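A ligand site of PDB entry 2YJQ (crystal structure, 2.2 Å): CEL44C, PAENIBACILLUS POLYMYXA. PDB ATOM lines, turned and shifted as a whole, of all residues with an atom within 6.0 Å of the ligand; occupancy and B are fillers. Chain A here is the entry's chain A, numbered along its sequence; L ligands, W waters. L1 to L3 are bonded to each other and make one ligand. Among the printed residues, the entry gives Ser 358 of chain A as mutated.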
ATOM      1  N   GLY A  46     -12.138   7.707 -16.768  1.00  0.00           N
ATOM      2  CA  GLY A  46     -13.076   8.780 -16.462  1.00  0.00           C
ATOM      3  C   GLY A  46     -13.000   8.992 -14.963  1.00  0.00           C
ATOM      4  O   GLY A  46     -12.044   8.543 -14.316  1.00  0.00           O
ATOM      5  N   GLY A  47     -14.012   9.608 -14.365  1.00  0.00           N
ATOM      6  CA  GLY A  47     -13.987   9.987 -12.944  1.00  0.00           C
ATOM      7  C   GLY A  47     -13.383  11.361 -12.674  1.00  0.00           C
ATOM      8  O   GLY A  47     -12.870  12.061 -13.580  1.00  0.00           O
ATOM      9  N   ASN A  48     -13.453  11.784 -11.418  1.00  0.00           N
ATOM     10  CA  ASN A  48     -13.041  13.147 -10.977  1.00  0.00           C
ATOM     11  C   ASN A  48     -11.685  13.599 -11.515  1.00  0.00           C
ATOM     12  O   ASN A  48     -11.544  14.712 -12.006  1.00  0.00           O
ATOM     13  CB  ASN A  48     -13.089  13.201  -9.457  1.00  0.00           C
ATOM     14  CG  ASN A  48     -14.518  13.122  -8.945  1.00  0.00           C
ATOM     15  OD1 ASN A  48     -15.473  13.329  -9.718  1.00  0.00           O
ATOM     16  ND2 ASN A  48     -14.697  12.830  -7.658  1.00  0.00           N
ATOM     17  N   ARG A  49     -10.723  12.711 -11.508  1.00  0.00           N
ATOM     18  CA  ARG A  49      -9.373  13.076 -11.951  1.00  0.00           C
ATOM     19  C   ARG A  49      -9.229  13.490 -13.406  1.00  0.00           C
ATOM     20  O   ARG A  49      -8.274  14.253 -13.752  1.00  0.00           O
ATOM     21  CB  ARG A  49      -8.414  11.911 -11.644  1.00  0.00           C
ATOM     22  CG  ARG A  49      -7.871  11.909 -10.223  1.00  0.00           C
ATOM     23  CD  ARG A  49      -6.668  12.874 -10.135  1.00  0.00           C
ATOM     24  NE  ARG A  49      -5.999  12.970  -8.827  1.00  0.00           N
ATOM     25  CZ  ARG A  49      -4.841  13.647  -8.683  1.00  0.00           C
ATOM     26  NH1 ARG A  49      -4.255  14.220  -9.715  1.00  0.00           N
ATOM     27  NH2 ARG A  49      -4.244  13.704  -7.522  1.00  0.00           N
ATOM     28  N   MET A  50     -10.147  13.026 -14.274  1.00  0.00           N
ATOM     29  CA  MET A  50     -10.021  13.295 -15.728  1.00  0.00           C
ATOM     30  C   MET A  50     -10.457  14.695 -16.159  1.00  0.00           C
ATOM     31  O   MET A  50     -10.028  15.204 -17.207  1.00  0.00           O
ATOM     32  CB  MET A  50     -10.726  12.230 -16.583  1.00  0.00           C
ATOM     33  CG  MET A  50      -9.978  10.927 -16.638  1.00  0.00           C
ATOM     34  SD  MET A  50      -8.338  11.066 -17.312  1.00  0.00           S
ATOM     35  CE  MET A  50      -8.504  11.451 -19.064  1.00  0.00           C
ATOM     36  N   ASN A  61      -5.554  17.126 -11.465  1.00  0.00           N
ATOM     37  CA  ASN A  61      -5.854  17.681 -10.171  1.00  0.00           C
ATOM     38  C   ASN A  61      -6.946  16.934  -9.419  1.00  0.00           C
ATOM     39  O   ASN A  61      -7.998  16.640  -9.960  1.00  0.00           O
ATOM     40  CB  ASN A  61      -6.201  19.164 -10.326  1.00  0.00           C
ATOM     41  CG  ASN A  61      -6.263  19.898  -8.982  1.00  0.00           C
ATOM     42  OD1 ASN A  61      -7.194  19.665  -8.174  1.00  0.00           O
ATOM     43  ND2 ASN A  61      -5.254  20.777  -8.727  1.00  0.00           N
ATOM     44  N   ALA A  62      -6.710  16.688  -8.147  1.00  0.00           N
ATOM     45  CA  ALA A  62      -7.625  15.902  -7.319  1.00  0.00           C
ATOM     46  C   ALA A  62      -8.903  16.569  -6.932  1.00  0.00           C
ATOM     47  O   ALA A  62      -9.826  15.874  -6.435  1.00  0.00           O
ATOM     48  CB  ALA A  62      -6.912  15.452  -6.060  1.00  0.00           C
ATOM     49  N   ASP A  65     -11.312  15.667  -3.649  1.00  0.00           N
ATOM     50  CA  ASP A  65     -10.849  14.381  -3.165  1.00  0.00           C
ATOM     51  C   ASP A  65      -9.481  14.366  -2.386  1.00  0.00           C
ATOM     52  O   ASP A  65      -9.291  13.577  -1.502  1.00  0.00           O
ATOM     53  CB  ASP A  65     -10.804  13.393  -4.306  1.00  0.00           C
ATOM     54  CG  ASP A  65     -12.169  13.171  -4.947  1.00  0.00           C
ATOM     55  OD1 ASP A  65     -13.144  13.110  -4.219  1.00  0.00           O
ATOM     56  OD2 ASP A  65     -12.275  13.050  -6.189  1.00  0.00           O
ATOM     57  N   TRP A  66      -8.522  15.216  -2.737  1.00  0.00           N
ATOM     58  CA  TRP A  66      -7.230  15.287  -2.040  1.00  0.00           C
ATOM     59  C   TRP A  66      -6.665  16.679  -2.214  1.00  0.00           C
ATOM     60  O   TRP A  66      -5.833  16.892  -3.127  1.00  0.00           O
ATOM     61  CB  TRP A  66      -6.208  14.264  -2.609  1.00  0.00           C
ATOM     62  CG  TRP A  66      -4.889  14.186  -1.800  1.00  0.00           C
ATOM     63  CD1 TRP A  66      -4.777  14.055  -0.446  1.00  0.00           C
ATOM     64  CD2 TRP A  66      -3.538  14.215  -2.315  1.00  0.00           C
ATOM     65  NE1 TRP A  66      -3.431  14.005  -0.079  1.00  0.00           N
ATOM     66  CE2 TRP A  66      -2.651  14.105  -1.188  1.00  0.00           C
ATOM     67  CE3 TRP A  66      -2.979  14.310  -3.596  1.00  0.00           C
ATOM     68  CZ2 TRP A  66      -1.236  14.113  -1.312  1.00  0.00           C
ATOM     69  CZ3 TRP A  66      -1.536  14.310  -3.724  1.00  0.00           C
ATOM     70  CH2 TRP A  66      -0.688  14.213  -2.574  1.00  0.00           C
ATOM     71  N   SER A  69      -4.895  18.954  -5.122  1.00  0.00           N
ATOM     72  CA  SER A  69      -3.547  18.730  -5.514  1.00  0.00           C
ATOM     73  C   SER A  69      -3.437  18.483  -6.985  1.00  0.00           C
ATOM     74  O   SER A  69      -4.064  17.565  -7.498  1.00  0.00           O
ATOM     75  CB  SER A  69      -2.970  17.548  -4.752  1.00  0.00           C
ATOM     76  OG  SER A  69      -1.652  17.324  -5.217  1.00  0.00           O
ATOM     77  N   ASP A  71      -0.809  17.039  -9.521  1.00  0.00           N
ATOM     78  CA  ASP A  71       0.324  16.107  -9.376  1.00  0.00           C
ATOM     79  C   ASP A  71       0.287  14.994 -10.431  1.00  0.00           C
ATOM     80  O   ASP A  71      -0.577  15.016 -11.307  1.00  0.00           O
ATOM     81  CB  ASP A  71       0.287  15.533  -7.944  1.00  0.00           C
ATOM     82  CG  ASP A  71      -0.946  14.746  -7.708  1.00  0.00           C
ATOM     83  OD1 ASP A  71      -1.316  14.004  -8.632  1.00  0.00           O
ATOM     84  OD2 ASP A  71      -1.573  14.881  -6.649  1.00  0.00           O
ATOM     85  N   TYR A  73      -0.429  11.842 -10.136  1.00  0.00           N
ATOM     86  CA  TYR A  73      -1.214  10.690  -9.708  1.00  0.00           C
ATOM     87  C   TYR A  73      -1.659   9.760 -10.867  1.00  0.00           C
ATOM     88  O   TYR A  73      -1.601   8.559 -10.722  1.00  0.00           O
ATOM     89  CB  TYR A  73      -2.433  11.128  -8.891  1.00  0.00           C
ATOM     90  CG  TYR A  73      -3.380  10.008  -8.546  1.00  0.00           C
ATOM     91  CD1 TYR A  73      -3.123   9.138  -7.455  1.00  0.00           C
ATOM     92  CD2 TYR A  73      -4.515   9.776  -9.305  1.00  0.00           C
ATOM     93  CE1 TYR A  73      -4.038   8.102  -7.108  1.00  0.00           C
ATOM     94  CE2 TYR A  73      -5.414   8.760  -8.992  1.00  0.00           C
ATOM     95  CZ  TYR A  73      -5.173   7.937  -7.896  1.00  0.00           C
ATOM     96  OH  TYR A  73      -6.073   6.956  -7.637  1.00  0.00           O
ATOM     97  N   ASN A 186     -16.919  14.997 -16.852  1.00  0.00           N
ATOM     98  CA  ASN A 186     -17.338  14.085 -15.813  1.00  0.00           C
ATOM     99  C   ASN A 186     -18.088  14.879 -14.790  1.00  0.00           C
ATOM    100  O   ASN A 186     -17.592  15.918 -14.349  1.00  0.00           O
ATOM    101  CB  ASN A 186     -16.118  13.423 -15.130  1.00  0.00           C
ATOM    102  CG  ASN A 186     -16.495  12.489 -13.980  1.00  0.00           C
ATOM    103  OD1 ASN A 186     -16.553  12.902 -12.798  1.00  0.00           O
ATOM    104  ND2 ASN A 186     -16.741  11.236 -14.304  1.00  0.00           N
ATOM    105  N   GLU A 187     -19.239  14.379 -14.374  1.00  0.00           N
ATOM    106  CA  GLU A 187     -20.095  15.045 -13.370  1.00  0.00           C
ATOM    107  C   GLU A 187     -20.097  16.590 -13.349  1.00  0.00           C
ATOM    108  O   GLU A 187     -19.814  17.243 -12.325  1.00  0.00           O
ATOM    109  CB  GLU A 187     -19.887  14.446 -11.989  1.00  0.00           C
ATOM    110  CG  GLU A 187     -19.772  12.913 -12.063  1.00  0.00           C
ATOM    111  CD  GLU A 187     -19.627  12.238 -10.738  1.00  0.00           C
ATOM    112  OE1 GLU A 187     -19.195  12.930  -9.790  1.00  0.00           O
ATOM    113  OE2 GLU A 187     -19.930  11.028 -10.651  1.00  0.00           O
ATOM    114  N   HIS A 284     -24.198   8.230 -14.040  1.00  0.00           N
ATOM    115  CA  HIS A 284     -23.654   7.437 -12.961  1.00  0.00           C
ATOM    116  C   HIS A 284     -24.782   7.201 -11.987  1.00  0.00           C
ATOM    117  O   HIS A 284     -25.691   8.026 -11.848  1.00  0.00           O
ATOM    118  CB  HIS A 284     -22.519   8.156 -12.274  1.00  0.00           C
ATOM    119  CG  HIS A 284     -21.372   8.465 -13.184  1.00  0.00           C
ATOM    120  ND1 HIS A 284     -20.353   9.326 -12.837  1.00  0.00           N
ATOM    121  CD2 HIS A 284     -21.081   8.018 -14.437  1.00  0.00           C
ATOM    122  CE1 HIS A 284     -19.497   9.430 -13.834  1.00  0.00           C
ATOM    123  NE2 HIS A 284     -19.913   8.641 -14.817  1.00  0.00           N
ATOM    124  N   TYR A 286     -24.991   5.671  -8.128  1.00  0.00           N
ATOM    125  CA  TYR A 286     -24.573   5.102  -6.845  1.00  0.00           C
ATOM    126  C   TYR A 286     -25.816   5.068  -6.013  1.00  0.00           C
ATOM    127  O   TYR A 286     -26.327   6.132  -5.712  1.00  0.00           O
ATOM    128  CB  TYR A 286     -23.560   6.023  -6.185  1.00  0.00           C
ATOM    129  CG  TYR A 286     -22.309   6.210  -7.035  1.00  0.00           C
ATOM    130  CD1 TYR A 286     -21.359   5.187  -7.171  1.00  0.00           C
ATOM    131  CD2 TYR A 286     -22.115   7.409  -7.720  1.00  0.00           C
ATOM    132  CE1 TYR A 286     -20.212   5.368  -7.971  1.00  0.00           C
ATOM    133  CE2 TYR A 286     -20.976   7.607  -8.507  1.00  0.00           C
ATOM    134  CZ  TYR A 286     -20.029   6.599  -8.618  1.00  0.00           C
ATOM    135  OH  TYR A 286     -18.916   6.826  -9.437  1.00  0.00           O
ATOM    136  N   SER A 358     -20.562   4.657 -14.462  1.00  0.00           N
ATOM    137  CA  SER A 358     -19.845   4.522 -13.212  1.00  0.00           C
ATOM    138  C   SER A 358     -20.915   4.198 -12.180  1.00  0.00           C
ATOM    139  O   SER A 358     -21.807   5.020 -11.979  1.00  0.00           O
ATOM    140  CB  SER A 358     -19.137   5.863 -12.899  1.00  0.00           C
ATOM    141  OG  SER A 358     -18.205   5.683 -11.865  1.00  0.00           O
ATOM    142  N   TRP A 391     -17.523   0.885 -10.865  1.00  0.00           N
ATOM    143  CA  TRP A 391     -16.585   1.799 -10.233  1.00  0.00           C
ATOM    144  C   TRP A 391     -16.167   1.298  -8.827  1.00  0.00           C
ATOM    145  O   TRP A 391     -17.025   0.952  -8.014  1.00  0.00           O
ATOM    146  CB  TRP A 391     -17.129   3.238 -10.176  1.00  0.00           C
ATOM    147  CG  TRP A 391     -16.184   4.128  -9.482  1.00  0.00           C
ATOM    148  CD1 TRP A 391     -16.107   4.329  -8.150  1.00  0.00           C
ATOM    149  CD2 TRP A 391     -15.114   4.877 -10.074  1.00  0.00           C
ATOM    150  NE1 TRP A 391     -15.086   5.190  -7.849  1.00  0.00           N
ATOM    151  CE2 TRP A 391     -14.439   5.537  -9.011  1.00  0.00           C
ATOM    152  CE3 TRP A 391     -14.675   5.106 -11.400  1.00  0.00           C
ATOM    153  CZ2 TRP A 391     -13.339   6.393  -9.220  1.00  0.00           C
ATOM    154  CZ3 TRP A 391     -13.573   5.916 -11.618  1.00  0.00           C
ATOM    155  CH2 TRP A 391     -12.915   6.571 -10.542  1.00  0.00           C
ATOM    156  N   LYS A 392     -14.862   1.234  -8.561  1.00  0.00           N
ATOM    157  CA  LYS A 392     -14.365   0.795  -7.264  1.00  0.00           C
ATOM    158  C   LYS A 392     -14.468   1.903  -6.199  1.00  0.00           C
ATOM    159  O   LYS A 392     -13.740   2.887  -6.269  1.00  0.00           O
ATOM    160  CB  LYS A 392     -12.907   0.248  -7.363  1.00  0.00           C
ATOM    161  CG  LYS A 392     -12.714  -1.028  -8.204  1.00  0.00           C
ATOM    162  CD  LYS A 392     -11.241  -1.355  -8.360  1.00  0.00           C
ATOM    163  CE  LYS A 392     -10.729  -2.052  -7.121  1.00  0.00           C
ATOM    164  NZ  LYS A 392      -9.219  -2.144  -7.164  1.00  0.00           N
ATOM    165  N   LEU A 393     -15.364   1.719  -5.229  1.00  0.00           N
ATOM    166  CA  LEU A 393     -15.482   2.660  -4.116  1.00  0.00           C
ATOM    167  C   LEU A 393     -14.536   2.242  -3.000  1.00  0.00           C
ATOM    168  O   LEU A 393     -14.283   3.009  -2.093  1.00  0.00           O
ATOM    169  CB  LEU A 393     -16.927   2.758  -3.557  1.00  0.00           C
ATOM    170  CG  LEU A 393     -18.031   3.267  -4.499  1.00  0.00           C
ATOM    171  CD1 LEU A 393     -19.384   2.932  -3.900  1.00  0.00           C
ATOM    172  CD2 LEU A 393     -17.947   4.760  -4.983  1.00  0.00           C
ATOM    173  N   ASP A 395     -10.619   0.503  -2.423  1.00  0.00           N
ATOM    174  CA  ASP A 395      -9.307   0.054  -2.850  1.00  0.00           C
ATOM    175  C   ASP A 395      -9.056  -1.421  -2.525  1.00  0.00           C
ATOM    176  O   ASP A 395      -9.740  -2.010  -1.680  1.00  0.00           O
ATOM    177  CB  ASP A 395      -8.230   0.919  -2.220  1.00  0.00           C
ATOM    178  CG  ASP A 395      -8.251   2.333  -2.740  1.00  0.00           C
ATOM    179  OD1 ASP A 395      -8.865   2.571  -3.807  1.00  0.00           O
ATOM    180  OD2 ASP A 395      -7.646   3.204  -2.097  1.00  0.00           O
HETATM  181  C1  LIG L   1      -7.664  11.340  -5.666  1.00  0.00           C
HETATM  182  C2  LIG L   1      -6.207  10.990  -5.275  1.00  0.00           C
HETATM  183  C3  LIG L   1      -6.164  10.218  -3.975  1.00  0.00           C
HETATM  184  C4  LIG L   1      -7.095   9.028  -4.122  1.00  0.00           C
HETATM  185  C5  LIG L   1      -6.908   8.132  -2.897  1.00  0.00           C
HETATM  186  C6  LIG L   1      -8.506  10.089  -5.662  1.00  0.00           C
HETATM  187  O1  LIG L   1      -7.741  11.957  -6.961  1.00  0.00           O
HETATM  188  O2  LIG L   1      -5.422  12.152  -5.106  1.00  0.00           O
HETATM  189  O3  LIG L   1      -4.837   9.695  -3.860  1.00  0.00           O
HETATM  190  O4  LIG L   1      -8.405   9.573  -4.353  1.00  0.00           O
HETATM  191  O5  LIG L   1      -8.080   8.048  -2.097  1.00  0.00           O
HETATM  192  C1  LG2 L   2     -12.986   8.738  -5.279  1.00  0.00           C
HETATM  193  C2  LG2 L   2     -11.759   9.543  -4.876  1.00  0.00           C
HETATM  194  C3  LG2 L   2     -10.787   9.561  -6.054  1.00  0.00           C
HETATM  195  C4  LG2 L   2     -11.425   9.919  -7.390  1.00  0.00           C
HETATM  196  C5  LG2 L   2     -10.457   9.648  -8.542  1.00  0.00           C
HETATM  197  C6  LG2 L   2     -13.604   9.312  -6.575  1.00  0.00           C
HETATM  198  O1  LG2 L   2     -13.966   8.789  -4.246  1.00  0.00           O
HETATM  199  O2  LG2 L   2     -11.089   8.763  -3.884  1.00  0.00           O
HETATM  200  O3  LG2 L   2      -9.833  10.544  -5.901  1.00  0.00           O
HETATM  201  O4  LG2 L   2     -12.615   9.149  -7.612  1.00  0.00           O
HETATM  202  O5  LG2 L   2     -11.166  10.094  -9.704  1.00  0.00           O
HETATM  203  C1  LG3 L   3     -17.462   8.635  -5.584  1.00  0.00           C
HETATM  204  C2  LG3 L   3     -17.178   8.467  -7.080  1.00  0.00           C
HETATM  205  C3  LG3 L   3     -15.847   9.154  -7.561  1.00  0.00           C
HETATM  206  C4  LG3 L   3     -15.674   9.116  -9.076  1.00  0.00           C
HETATM  207  C5  LG3 L   3     -16.897   9.715  -9.828  1.00  0.00           C
HETATM  208  O1  LG3 L   3     -17.441  10.061  -5.293  1.00  0.00           O
HETATM  209  O2  LG3 L   3     -18.215   9.149  -7.802  1.00  0.00           O
HETATM  210  O3  LG3 L   3     -14.738   8.488  -6.946  1.00  0.00           O
HETATM  211  O4  LG3 L   3     -14.443   9.745  -9.522  1.00  0.00           O
HETATM  212  N1  LG3 L   3     -18.110   9.151  -9.196  1.00  0.00           N
HETATM  213  O   HOH W   1     -16.347   7.587 -12.388  1.00  0.00           O
HETATM  214  O   HOH W   2     -10.527   8.972 -11.885  1.00  0.00           O
HETATM  215  O   HOH W   3     -18.672  12.360  -6.950  1.00  0.00           O
HETATM  216  O   HOH W   4     -15.070  11.365  -4.284  1.00  0.00           O
HETATM  217  O   HOH W   5      -6.705   6.928   0.588  1.00  0.00           O
HETATM  218  O   HOH W   6     -10.100  13.140  -7.598  1.00  0.00           O
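The side-chain carboxylate (OE2) of Glu 187 is in hydrogen-bond range of a nitrogen (N1) of LG3 L3 (3.0 Å). The indole nitrogen of Trp 391 lies close to an oxygen (O3) of LG3 L3, at 3.4 Å. The side-chain hydroxyl of Tyr 286 lies within hydrogen-bond range of a nitrogen (N1) of LG3 L3, at 2.5 Å. O1 of LIG L1 is in hydrogen-bond range of NE of Arg 49, at 2.7 Å. The backbone NH of Asn 48 sits at hydrogen-bond distance from an oxygen (O4) of LG3 L3 (3.0 Å). The backbone NH (N) of Arg 49 sits at hydrogen-bond distance from an oxygen (O5) of LG2 L2 (3.2 Å).
The side-chain carboxylate of Asp 65 sits at hydrogen-bond distance from the side-chain amide nitrogen of Asn 48, 2.8 Å away. OD1 of Asp 71 sits at hydrogen-bond distance from N of Tyr 73, at 2.8 Å. OE2 of Glu 187 sits at hydrogen-bond distance from ND1 of His 284 (2.8 Å). OD1 of Asn 48 sits close to OD1 of Asn 186 (3.3 Å). N of Ala 62 lies within hydrogen-bond range of O of Ser 69, 2.9 Å away. The side-chain hydroxyl (OG) of Ser 358 lies within hydrogen-bond range of the side-chain hydroxyl (OH) of Tyr 286 (2.8 Å). The backbone NH of Gly 47 sits close to the side-chain amide nitrogen of Asn 186 (3.2 Å). The guanidinium group (NH2) of Arg 49 is in salt-bridge range of the side-chain carboxylate (OD2) of Asp 71 (3.0 Å).
Residues that only touch the ligand: Trp 66 (3.4 Å), Asp 65 (3.4 Å), Gly 47 (3.5 Å), Ala 62 (3.7 Å), Tyr 73 (3.7 Å) and Leu 393 (3.95 Å). The nearest printed residue that does not touch the ligand is His 284 (4.3 Å).
Water W2 lies within hydrogen-bond range of an oxygen (O5) of LG2 L2 (2.5 Å) and the backbone carbonyl oxygen (O) of Gly 46 (2.9 Å). Water W6 lies within hydrogen-bond range of the side-chain carboxylate of Asp 65 (2.6 Å), an oxygen (O1) of LIG L1 (2.7 Å) and the backbone carbonyl oxygen of Ala 62 (3.0 Å). Water W4 lies within hydrogen-bond range of OD1 of Asp 65 (2.6 Å) and O1 of LG2 L2 (2.8 Å). Water W3 lies within hydrogen-bond range of OE1 of Glu 187 (2.9 Å) and O1 of LG3 L3 (3.1 Å).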
